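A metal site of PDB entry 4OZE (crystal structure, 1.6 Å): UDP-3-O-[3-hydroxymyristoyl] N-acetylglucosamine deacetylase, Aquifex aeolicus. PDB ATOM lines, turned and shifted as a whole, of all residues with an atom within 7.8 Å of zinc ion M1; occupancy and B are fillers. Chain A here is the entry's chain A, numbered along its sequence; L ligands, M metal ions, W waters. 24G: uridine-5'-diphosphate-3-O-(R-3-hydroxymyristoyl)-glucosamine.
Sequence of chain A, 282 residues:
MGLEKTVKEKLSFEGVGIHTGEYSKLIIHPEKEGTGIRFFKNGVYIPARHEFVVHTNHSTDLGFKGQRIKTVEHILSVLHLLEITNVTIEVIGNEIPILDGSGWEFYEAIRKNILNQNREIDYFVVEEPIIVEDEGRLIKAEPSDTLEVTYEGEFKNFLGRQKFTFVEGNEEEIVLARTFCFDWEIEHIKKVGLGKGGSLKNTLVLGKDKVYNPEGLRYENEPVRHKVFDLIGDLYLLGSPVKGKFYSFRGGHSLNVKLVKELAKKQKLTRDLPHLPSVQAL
Zinc ion M1 is bound by water W1, 1.9 Å away.
Zinc ion M1 is bound by OD1 of Asp 230, 2.0 Å away.
A ring nitrogen (NE2) of His 226 binds zinc ion M1.
Zinc ion M1 is bound by NE2 of His 74, at 2.0 Å.
Slightly farther from zinc ion M1 lies OD2 of Asp 230 (2.8 Å).
O9 of the ligand sits at hydrogen-bond distance from O of Phe 180 (2.6 Å).
A nitrogen (N11) of the ligand lies close to the backbone carbonyl oxygen (O) of His 58 (2.8 Å).
The side-chain hydroxyl of Thr 179 lies within hydrogen-bond range of an oxygen (O10) of the ligand (3.3 Å).
The backbone NH of His 253 sits at hydrogen-bond distance from an oxygen (O18) of the ligand (2.9 Å).
NZ of Lys 227 is in salt-bridge range of O22 of the ligand (2.8 Å).
Three residues have an atom within 4 Å of zinc ion M1: His 74, His 226 and Asp 230.
A ring nitrogen (ND1) of His 226 is in hydrogen-bond range of the backbone carbonyl oxygen (O) of Ala 177, at 2.8 Å.
The backbone carbonyl oxygen (O) of Arg 178 lies close to a ring nitrogen (ND1) of His 226 (3.4 Å).
N of Thr 179 sits at hydrogen-bond distance from ND1 of His 226, 3.3 Å away.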
ATOM      1  N   HIS A  58       5.007 -15.800  -2.504  1.00  0.00           N
ATOM      2  CA  HIS A  58       6.391 -15.861  -2.035  1.00  0.00           C
ATOM      3  C   HIS A  58       7.316 -14.877  -2.769  1.00  0.00           C
ATOM      4  O   HIS A  58       8.521 -14.921  -2.566  1.00  0.00           O
ATOM      5  CB  HIS A  58       6.981 -17.297  -2.071  1.00  0.00           C
ATOM      6  CG  HIS A  58       6.137 -18.279  -1.310  1.00  0.00           C
ATOM      7  ND1 HIS A  58       6.129 -18.295   0.067  1.00  0.00           N
ATOM      8  CD2 HIS A  58       5.239 -19.185  -1.768  1.00  0.00           C
ATOM      9  CE1 HIS A  58       5.253 -19.223   0.404  1.00  0.00           C
ATOM     10  NE2 HIS A  58       4.679 -19.773  -0.667  1.00  0.00           N
ATOM     11  N   SER A  59       6.746 -13.995  -3.597  1.00  0.00           N
ATOM     12  CA  SER A  59       7.457 -12.958  -4.336  1.00  0.00           C
ATOM     13  C   SER A  59       6.442 -12.166  -5.110  1.00  0.00           C
ATOM     14  O   SER A  59       5.319 -12.604  -5.254  1.00  0.00           O
ATOM     15  CB  SER A  59       8.490 -13.541  -5.296  1.00  0.00           C
ATOM     16  OG  SER A  59       7.927 -14.430  -6.253  1.00  0.00           O
ATOM     17  N   THR A  71      10.153 -11.934  -8.767  1.00  0.00           N
ATOM     18  CA  THR A  71      10.850 -11.301  -7.646  1.00  0.00           C
ATOM     19  C   THR A  71      11.283  -9.866  -7.961  1.00  0.00           C
ATOM     20  O   THR A  71      12.476  -9.539  -7.875  1.00  0.00           O
ATOM     21  CB  THR A  71      11.995 -12.225  -7.187  1.00  0.00           C
ATOM     22  OG1 THR A  71      11.504 -13.600  -7.194  1.00  0.00           O
ATOM     23  CG2 THR A  71      12.536 -11.840  -5.788  1.00  0.00           C
ATOM     24  N   GLU A  73      10.314  -7.181  -6.239  1.00  0.00           N
ATOM     25  CA  GLU A  73      10.119  -6.313  -5.072  1.00  0.00           C
ATOM     26  C   GLU A  73      11.336  -5.510  -4.623  1.00  0.00           C
ATOM     27  O   GLU A  73      11.164  -4.356  -4.196  1.00  0.00           O
ATOM     28  CB  GLU A  73       9.541  -7.111  -3.856  1.00  0.00           C
ATOM     29  CG  GLU A  73      10.314  -8.363  -3.477  1.00  0.00           C
ATOM     30  CD  GLU A  73       9.764  -9.669  -4.031  1.00  0.00           C
ATOM     31  OE1 GLU A  73       9.338  -9.665  -5.208  1.00  0.00           O
ATOM     32  OE2 GLU A  73       9.865 -10.710  -3.350  1.00  0.00           O
ATOM     33  N   HIS A  74      12.520  -6.088  -4.696  1.00  0.00           N
ATOM     34  CA  HIS A  74      13.711  -5.399  -4.176  1.00  0.00           C
ATOM     35  C   HIS A  74      14.243  -4.348  -5.123  1.00  0.00           C
ATOM     36  O   HIS A  74      14.544  -3.230  -4.671  1.00  0.00           O
ATOM     37  CB  HIS A  74      14.799  -6.409  -3.774  1.00  0.00           C
ATOM     38  CG  HIS A  74      14.334  -7.379  -2.729  1.00  0.00           C
ATOM     39  ND1 HIS A  74      15.053  -8.531  -2.435  1.00  0.00           N
ATOM     40  CD2 HIS A  74      13.225  -7.369  -1.937  1.00  0.00           C
ATOM     41  CE1 HIS A  74      14.371  -9.153  -1.480  1.00  0.00           C
ATOM     42  NE2 HIS A  74      13.241  -8.523  -1.186  1.00  0.00           N
ATOM     43  N   SER A  77      11.850  -1.517  -4.879  1.00  0.00           N
ATOM     44  CA  SER A  77      11.923  -0.739  -3.634  1.00  0.00           C
ATOM     45  C   SER A  77      13.065   0.258  -3.713  1.00  0.00           C
ATOM     46  O   SER A  77      12.864   1.426  -3.387  1.00  0.00           O
ATOM     47  CB  SER A  77      12.128  -1.642  -2.432  1.00  0.00           C
ATOM     48  OG  SER A  77      11.997  -0.838  -1.258  1.00  0.00           O
ATOM     49  N   ILE A  98      18.868 -12.280  -6.689  1.00  0.00           N
ATOM     50  CA  ILE A  98      18.593 -11.991  -5.266  1.00  0.00           C
ATOM     51  C   ILE A  98      19.777 -11.293  -4.598  1.00  0.00           C
ATOM     52  O   ILE A  98      19.583 -10.563  -3.602  1.00  0.00           O
ATOM     53  CB  ILE A  98      18.164 -13.280  -4.518  1.00  0.00           C
ATOM     54  CG1 ILE A  98      17.648 -12.954  -3.082  1.00  0.00           C
ATOM     55  CG2 ILE A  98      19.308 -14.343  -4.456  1.00  0.00           C
ATOM     56  CD1 ILE A  98      16.353 -12.167  -3.039  1.00  0.00           C
ATOM     57  N   GLY A 101      20.087 -10.824  -0.689  1.00  0.00           N
ATOM     58  CA  GLY A 101      18.746 -10.850  -0.136  1.00  0.00           C
ATOM     59  C   GLY A 101      18.227  -9.497   0.325  1.00  0.00           C
ATOM     60  O   GLY A 101      17.110  -9.407   0.802  1.00  0.00           O
ATOM     61  N   SER A 102      19.055  -8.440   0.154  1.00  0.00           N
ATOM     62  CA  SER A 102      18.681  -7.067   0.528  1.00  0.00           C
ATOM     63  C   SER A 102      18.741  -6.152  -0.721  1.00  0.00           C
ATOM     64  O   SER A 102      19.019  -6.633  -1.827  1.00  0.00           O
ATOM     65  CB  SER A 102      19.656  -6.535   1.592  1.00  0.00           C
ATOM     66  OG  SER A 102      20.894  -6.142   1.042  1.00  0.00           O
ATOM     67  N   ALA A 177      18.553  -4.652   5.067  1.00  0.00           N
ATOM     68  CA  ALA A 177      17.749  -5.714   5.714  1.00  0.00           C
ATOM     69  C   ALA A 177      17.444  -6.836   4.716  1.00  0.00           C
ATOM     70  O   ALA A 177      16.902  -6.572   3.634  1.00  0.00           O
ATOM     71  CB  ALA A 177      16.468  -5.121   6.305  1.00  0.00           C
ATOM     72  N   ARG A 178      17.810  -8.066   5.075  1.00  0.00           N
ATOM     73  CA  ARG A 178      17.649  -9.204   4.168  1.00  0.00           C
ATOM     74  C   ARG A 178      16.350  -9.956   4.268  1.00  0.00           C
ATOM     75  O   ARG A 178      15.697  -9.978   5.323  1.00  0.00           O
ATOM     76  CB  ARG A 178      18.780 -10.208   4.408  1.00  0.00           C
ATOM     77  CG  ARG A 178      20.153  -9.640   4.137  1.00  0.00           C
ATOM     78  CD  ARG A 178      21.154 -10.578   4.741  1.00  0.00           C
ATOM     79  NE  ARG A 178      21.171 -10.420   6.187  1.00  0.00           N
ATOM     80  CZ  ARG A 178      21.883 -11.167   7.017  1.00  0.00           C
ATOM     81  NH1 ARG A 178      22.593 -12.190   6.557  1.00  0.00           N
ATOM     82  NH2 ARG A 178      21.864 -10.909   8.330  1.00  0.00           N
ATOM     83  N   THR A 179      15.978 -10.614   3.162  1.00  0.00           N
ATOM     84  CA  THR A 179      14.801 -11.481   3.119  1.00  0.00           C
ATOM     85  C   THR A 179      15.026 -12.637   4.131  1.00  0.00           C
ATOM     86  O   THR A 179      16.179 -12.959   4.476  1.00  0.00           O
ATOM     87  CB  THR A 179      14.542 -12.013   1.713  1.00  0.00           C
ATOM     88  OG1 THR A 179      13.300 -12.741   1.753  1.00  0.00           O
ATOM     89  CG2 THR A 179      15.659 -12.910   1.219  1.00  0.00           C
ATOM     90  N   PHE A 180      13.936 -13.199   4.626  1.00  0.00           N
ATOM     91  CA  PHE A 180      14.039 -14.230   5.651  1.00  0.00           C
ATOM     92  C   PHE A 180      12.949 -15.258   5.503  1.00  0.00           C
ATOM     93  O   PHE A 180      11.908 -14.989   4.923  1.00  0.00           O
ATOM     94  CB  PHE A 180      13.957 -13.589   7.064  1.00  0.00           C
ATOM     95  CG  PHE A 180      12.624 -12.928   7.348  1.00  0.00           C
ATOM     96  CD1 PHE A 180      11.619 -13.606   8.043  1.00  0.00           C
ATOM     97  CD2 PHE A 180      12.353 -11.636   6.880  1.00  0.00           C
ATOM     98  CE1 PHE A 180      10.383 -12.993   8.307  1.00  0.00           C
ATOM     99  CE2 PHE A 180      11.102 -11.047   7.100  1.00  0.00           C
ATOM    100  CZ  PHE A 180      10.124 -11.713   7.836  1.00  0.00           C
ATOM    101  N   HIS A 226      12.983  -5.520   6.780  1.00  0.00           N
ATOM    102  CA  HIS A 226      12.843  -6.092   5.439  1.00  0.00           C
ATOM    103  C   HIS A 226      11.397  -5.994   4.930  1.00  0.00           C
ATOM    104  O   HIS A 226      11.181  -5.715   3.744  1.00  0.00           O
ATOM    105  CB  HIS A 226      13.291  -7.558   5.386  1.00  0.00           C
ATOM    106  CG  HIS A 226      13.356  -8.020   3.957  1.00  0.00           C
ATOM    107  ND1 HIS A 226      14.424  -7.670   3.125  1.00  0.00           N
ATOM    108  CD2 HIS A 226      12.397  -8.623   3.202  1.00  0.00           C
ATOM    109  CE1 HIS A 226      14.102  -8.126   1.925  1.00  0.00           C
ATOM    110  NE2 HIS A 226      12.905  -8.716   1.929  1.00  0.00           N
ATOM    111  N   LYS A 227      10.424  -6.244   5.805  1.00  0.00           N
ATOM    112  CA  LYS A 227       9.014  -6.181   5.379  1.00  0.00           C
ATOM    113  C   LYS A 227       8.632  -4.751   4.990  1.00  0.00           C
ATOM    114  O   LYS A 227       7.865  -4.574   4.018  1.00  0.00           O
ATOM    115  CB  LYS A 227       8.082  -6.705   6.480  1.00  0.00           C
ATOM    116  CG  LYS A 227       8.262  -8.208   6.757  1.00  0.00           C
ATOM    117  CD  LYS A 227       7.863  -9.069   5.572  1.00  0.00           C
ATOM    118  CE  LYS A 227       6.465  -9.570   5.718  1.00  0.00           C
ATOM    119  NZ  LYS A 227       6.140 -10.636   4.717  1.00  0.00           N
ATOM    120  N   PHE A 229      10.794  -2.619   3.631  1.00  0.00           N
ATOM    121  CA  PHE A 229      11.472  -2.519   2.340  1.00  0.00           C
ATOM    122  C   PHE A 229      10.619  -3.173   1.227  1.00  0.00           C
ATOM    123  O   PHE A 229      10.410  -2.588   0.153  1.00  0.00           O
ATOM    124  CB  PHE A 229      12.863  -3.178   2.481  1.00  0.00           C
ATOM    125  CG  PHE A 229      13.682  -3.201   1.224  1.00  0.00           C
ATOM    126  CD1 PHE A 229      14.276  -2.040   0.738  1.00  0.00           C
ATOM    127  CD2 PHE A 229      13.862  -4.394   0.521  1.00  0.00           C
ATOM    128  CE1 PHE A 229      15.032  -2.068  -0.441  1.00  0.00           C
ATOM    129  CE2 PHE A 229      14.661  -4.423  -0.630  1.00  0.00           C
ATOM    130  CZ  PHE A 229      15.242  -3.259  -1.114  1.00  0.00           C
ATOM    131  N   ASP A 230      10.035  -4.351   1.520  1.00  0.00           N
ATOM    132  CA  ASP A 230       9.160  -5.023   0.549  1.00  0.00           C
ATOM    133  C   ASP A 230       7.930  -4.176   0.229  1.00  0.00           C
ATOM    134  O   ASP A 230       7.541  -4.058  -0.941  1.00  0.00           O
ATOM    135  CB  ASP A 230       8.664  -6.335   1.126  1.00  0.00           C
ATOM    136  CG  ASP A 230       9.657  -7.484   0.991  1.00  0.00           C
ATOM    137  OD1 ASP A 230      10.609  -7.366   0.154  1.00  0.00           O
ATOM    138  OD2 ASP A 230       9.501  -8.488   1.710  1.00  0.00           O
ATOM    139  N   LEU A 231       7.288  -3.597   1.280  1.00  0.00           N
ATOM    140  CA  LEU A 231       6.069  -2.811   1.052  1.00  0.00           C
ATOM    141  C   LEU A 231       6.376  -1.590   0.183  1.00  0.00           C
ATOM    142  O   LEU A 231       5.560  -1.237  -0.698  1.00  0.00           O
ATOM    143  CB  LEU A 231       5.481  -2.402   2.404  1.00  0.00           C
ATOM    144  CG  LEU A 231       4.226  -1.496   2.397  1.00  0.00           C
ATOM    145  CD1 LEU A 231       3.152  -1.918   1.362  1.00  0.00           C
ATOM    146  CD2 LEU A 231       3.616  -1.464   3.785  1.00  0.00           C
ATOM    147  N   HIS A 253       3.347  -9.641   0.399  1.00  0.00           N
ATOM    148  CA  HIS A 253       3.133  -9.201  -0.992  1.00  0.00           C
ATOM    149  C   HIS A 253       1.672  -9.259  -1.445  1.00  0.00           C
ATOM    150  O   HIS A 253       1.213  -8.314  -2.077  1.00  0.00           O
ATOM    151  CB  HIS A 253       4.032  -9.971  -1.970  1.00  0.00           C
ATOM    152  CG  HIS A 253       5.495  -9.827  -1.695  1.00  0.00           C
ATOM    153  ND1 HIS A 253       6.117  -8.580  -1.696  1.00  0.00           N
ATOM    154  CD2 HIS A 253       6.442 -10.781  -1.490  1.00  0.00           C
ATOM    155  CE1 HIS A 253       7.407  -8.818  -1.456  1.00  0.00           C
ATOM    156  NE2 HIS A 253       7.643 -10.123  -1.341  1.00  0.00           N
HETATM  157  C36 24G L   1       4.127 -11.768   9.060  1.00  0.00           C
HETATM  158  C37 24G L   1       4.099 -12.932   8.391  1.00  0.00           C
HETATM  159  C35 24G L   1       4.017 -11.768  10.491  1.00  0.00           C
HETATM  160  C33 24G L   1       3.910 -14.237  10.412  1.00  0.00           C
HETATM  161  C13 24G L   1      10.722 -15.903   0.021  1.00  0.00           C
HETATM  162  C3  24G L   1       9.476 -12.836   0.693  1.00  0.00           C
HETATM  163  C2  24G L   1       9.679 -14.209   1.310  1.00  0.00           C
HETATM  164  C1  24G L   1       9.841 -14.159   2.827  1.00  0.00           C
HETATM  165  C26 24G L   1       3.348 -16.614   6.325  1.00  0.00           C
HETATM  166  C27 24G L   1       2.805 -15.522   7.253  1.00  0.00           C
HETATM  167  C25 24G L   1       4.858 -16.343   6.328  1.00  0.00           C
HETATM  168  C6  24G L   1       8.672 -13.407   3.458  1.00  0.00           C
HETATM  169  C28 24G L   1       3.933 -15.437   8.276  1.00  0.00           C
HETATM  170  C4  24G L   1       8.267 -12.067   1.452  1.00  0.00           C
HETATM  171  C52 24G L   1      21.800 -24.502   2.718  1.00  0.00           C
HETATM  172  C14 24G L   1      12.054 -16.475  -0.338  1.00  0.00           C
HETATM  173  C24 24G L   1       5.378 -15.566   5.137  1.00  0.00           C
HETATM  174  C7  24G L   1       8.876 -13.197   4.936  1.00  0.00           C
HETATM  175  C51 24G L   1      20.366 -24.519   3.154  1.00  0.00           C
HETATM  176  C50 24G L   1      19.730 -23.157   3.080  1.00  0.00           C
HETATM  177  C49 24G L   1      18.257 -23.143   3.360  1.00  0.00           C
HETATM  178  C48 24G L   1      17.571 -21.933   2.789  1.00  0.00           C
HETATM  179  C47 24G L   1      16.786 -22.223   1.564  1.00  0.00           C
HETATM  180  C46 24G L   1      15.312 -22.401   1.827  1.00  0.00           C
HETATM  181  C45 24G L   1      14.482 -22.200   0.602  1.00  0.00           C
HETATM  182  C44 24G L   1      14.567 -20.799   0.058  1.00  0.00           C
HETATM  183  C43 24G L   1      13.581 -19.908   0.669  1.00  0.00           C
HETATM  184  C42 24G L   1      13.479 -18.560  -0.002  1.00  0.00           C
HETATM  185  C40 24G L   1      12.194 -17.840   0.323  1.00  0.00           C
HETATM  186  N34 24G L   1       3.913 -13.025  11.064  1.00  0.00           N
HETATM  187  N32 24G L   1       3.982 -14.152   9.037  1.00  0.00           N
HETATM  188  N11 24G L   1       9.216 -12.871  -0.780  1.00  0.00           N
HETATM  189  O39 24G L   1       4.021 -10.778  11.223  1.00  0.00           O
HETATM  190  O38 24G L   1       3.876 -15.287  11.034  1.00  0.00           O
HETATM  191  O15 24G L   1       9.661 -16.429  -0.199  1.00  0.00           O
HETATM  192  O18 24G L   1       5.437 -11.114   1.707  1.00  0.00           O
HETATM  193  O21 24G L   1       3.157 -14.322   3.353  1.00  0.00           O
HETATM  194  O29 24G L   1       5.133 -15.615   7.559  1.00  0.00           O
HETATM  195  O5  24G L   1       8.530 -12.088   2.858  1.00  0.00           O
HETATM  196  O9  24G L   1       9.856 -15.477   3.360  1.00  0.00           O
HETATM  197  O30 24G L   1       3.065 -17.939   6.789  1.00  0.00           O
HETATM  198  O31 24G L   1       1.558 -15.846   7.842  1.00  0.00           O
HETATM  199  O8  24G L   1       7.701 -12.691   5.574  1.00  0.00           O
HETATM  200  O41 24G L   1      12.073 -17.662   1.728  1.00  0.00           O
HETATM  201  O17 24G L   1       4.671 -13.229   0.482  1.00  0.00           O
HETATM  202  O22 24G L   1       3.821 -12.115   4.452  1.00  0.00           O
HETATM  203  O10 24G L   1      10.862 -14.763   0.715  1.00  0.00           O
HETATM  204  O12 24G L   1       7.223 -12.843   1.123  1.00  0.00           O
HETATM  205  O23 24G L   1       4.878 -14.222   5.185  1.00  0.00           O
HETATM  206  O19 24G L   1       5.395 -13.309   2.911  1.00  0.00           O
HETATM  207  P16 24G L   1       5.512 -12.565   1.503  1.00  0.00           P
HETATM  208  P20 24G L   1       4.185 -13.454   3.953  1.00  0.00           P
HETATM  209 ZN    ZN M   1      11.843  -8.940   0.232  1.00  0.00          ZN
HETATM  210 ZN    ZN M   2       9.433 -10.899  -1.357  1.00  0.00          ZN
HETATM  211  O   HOH W   1      11.094 -10.560  -0.364  1.00  0.00           O
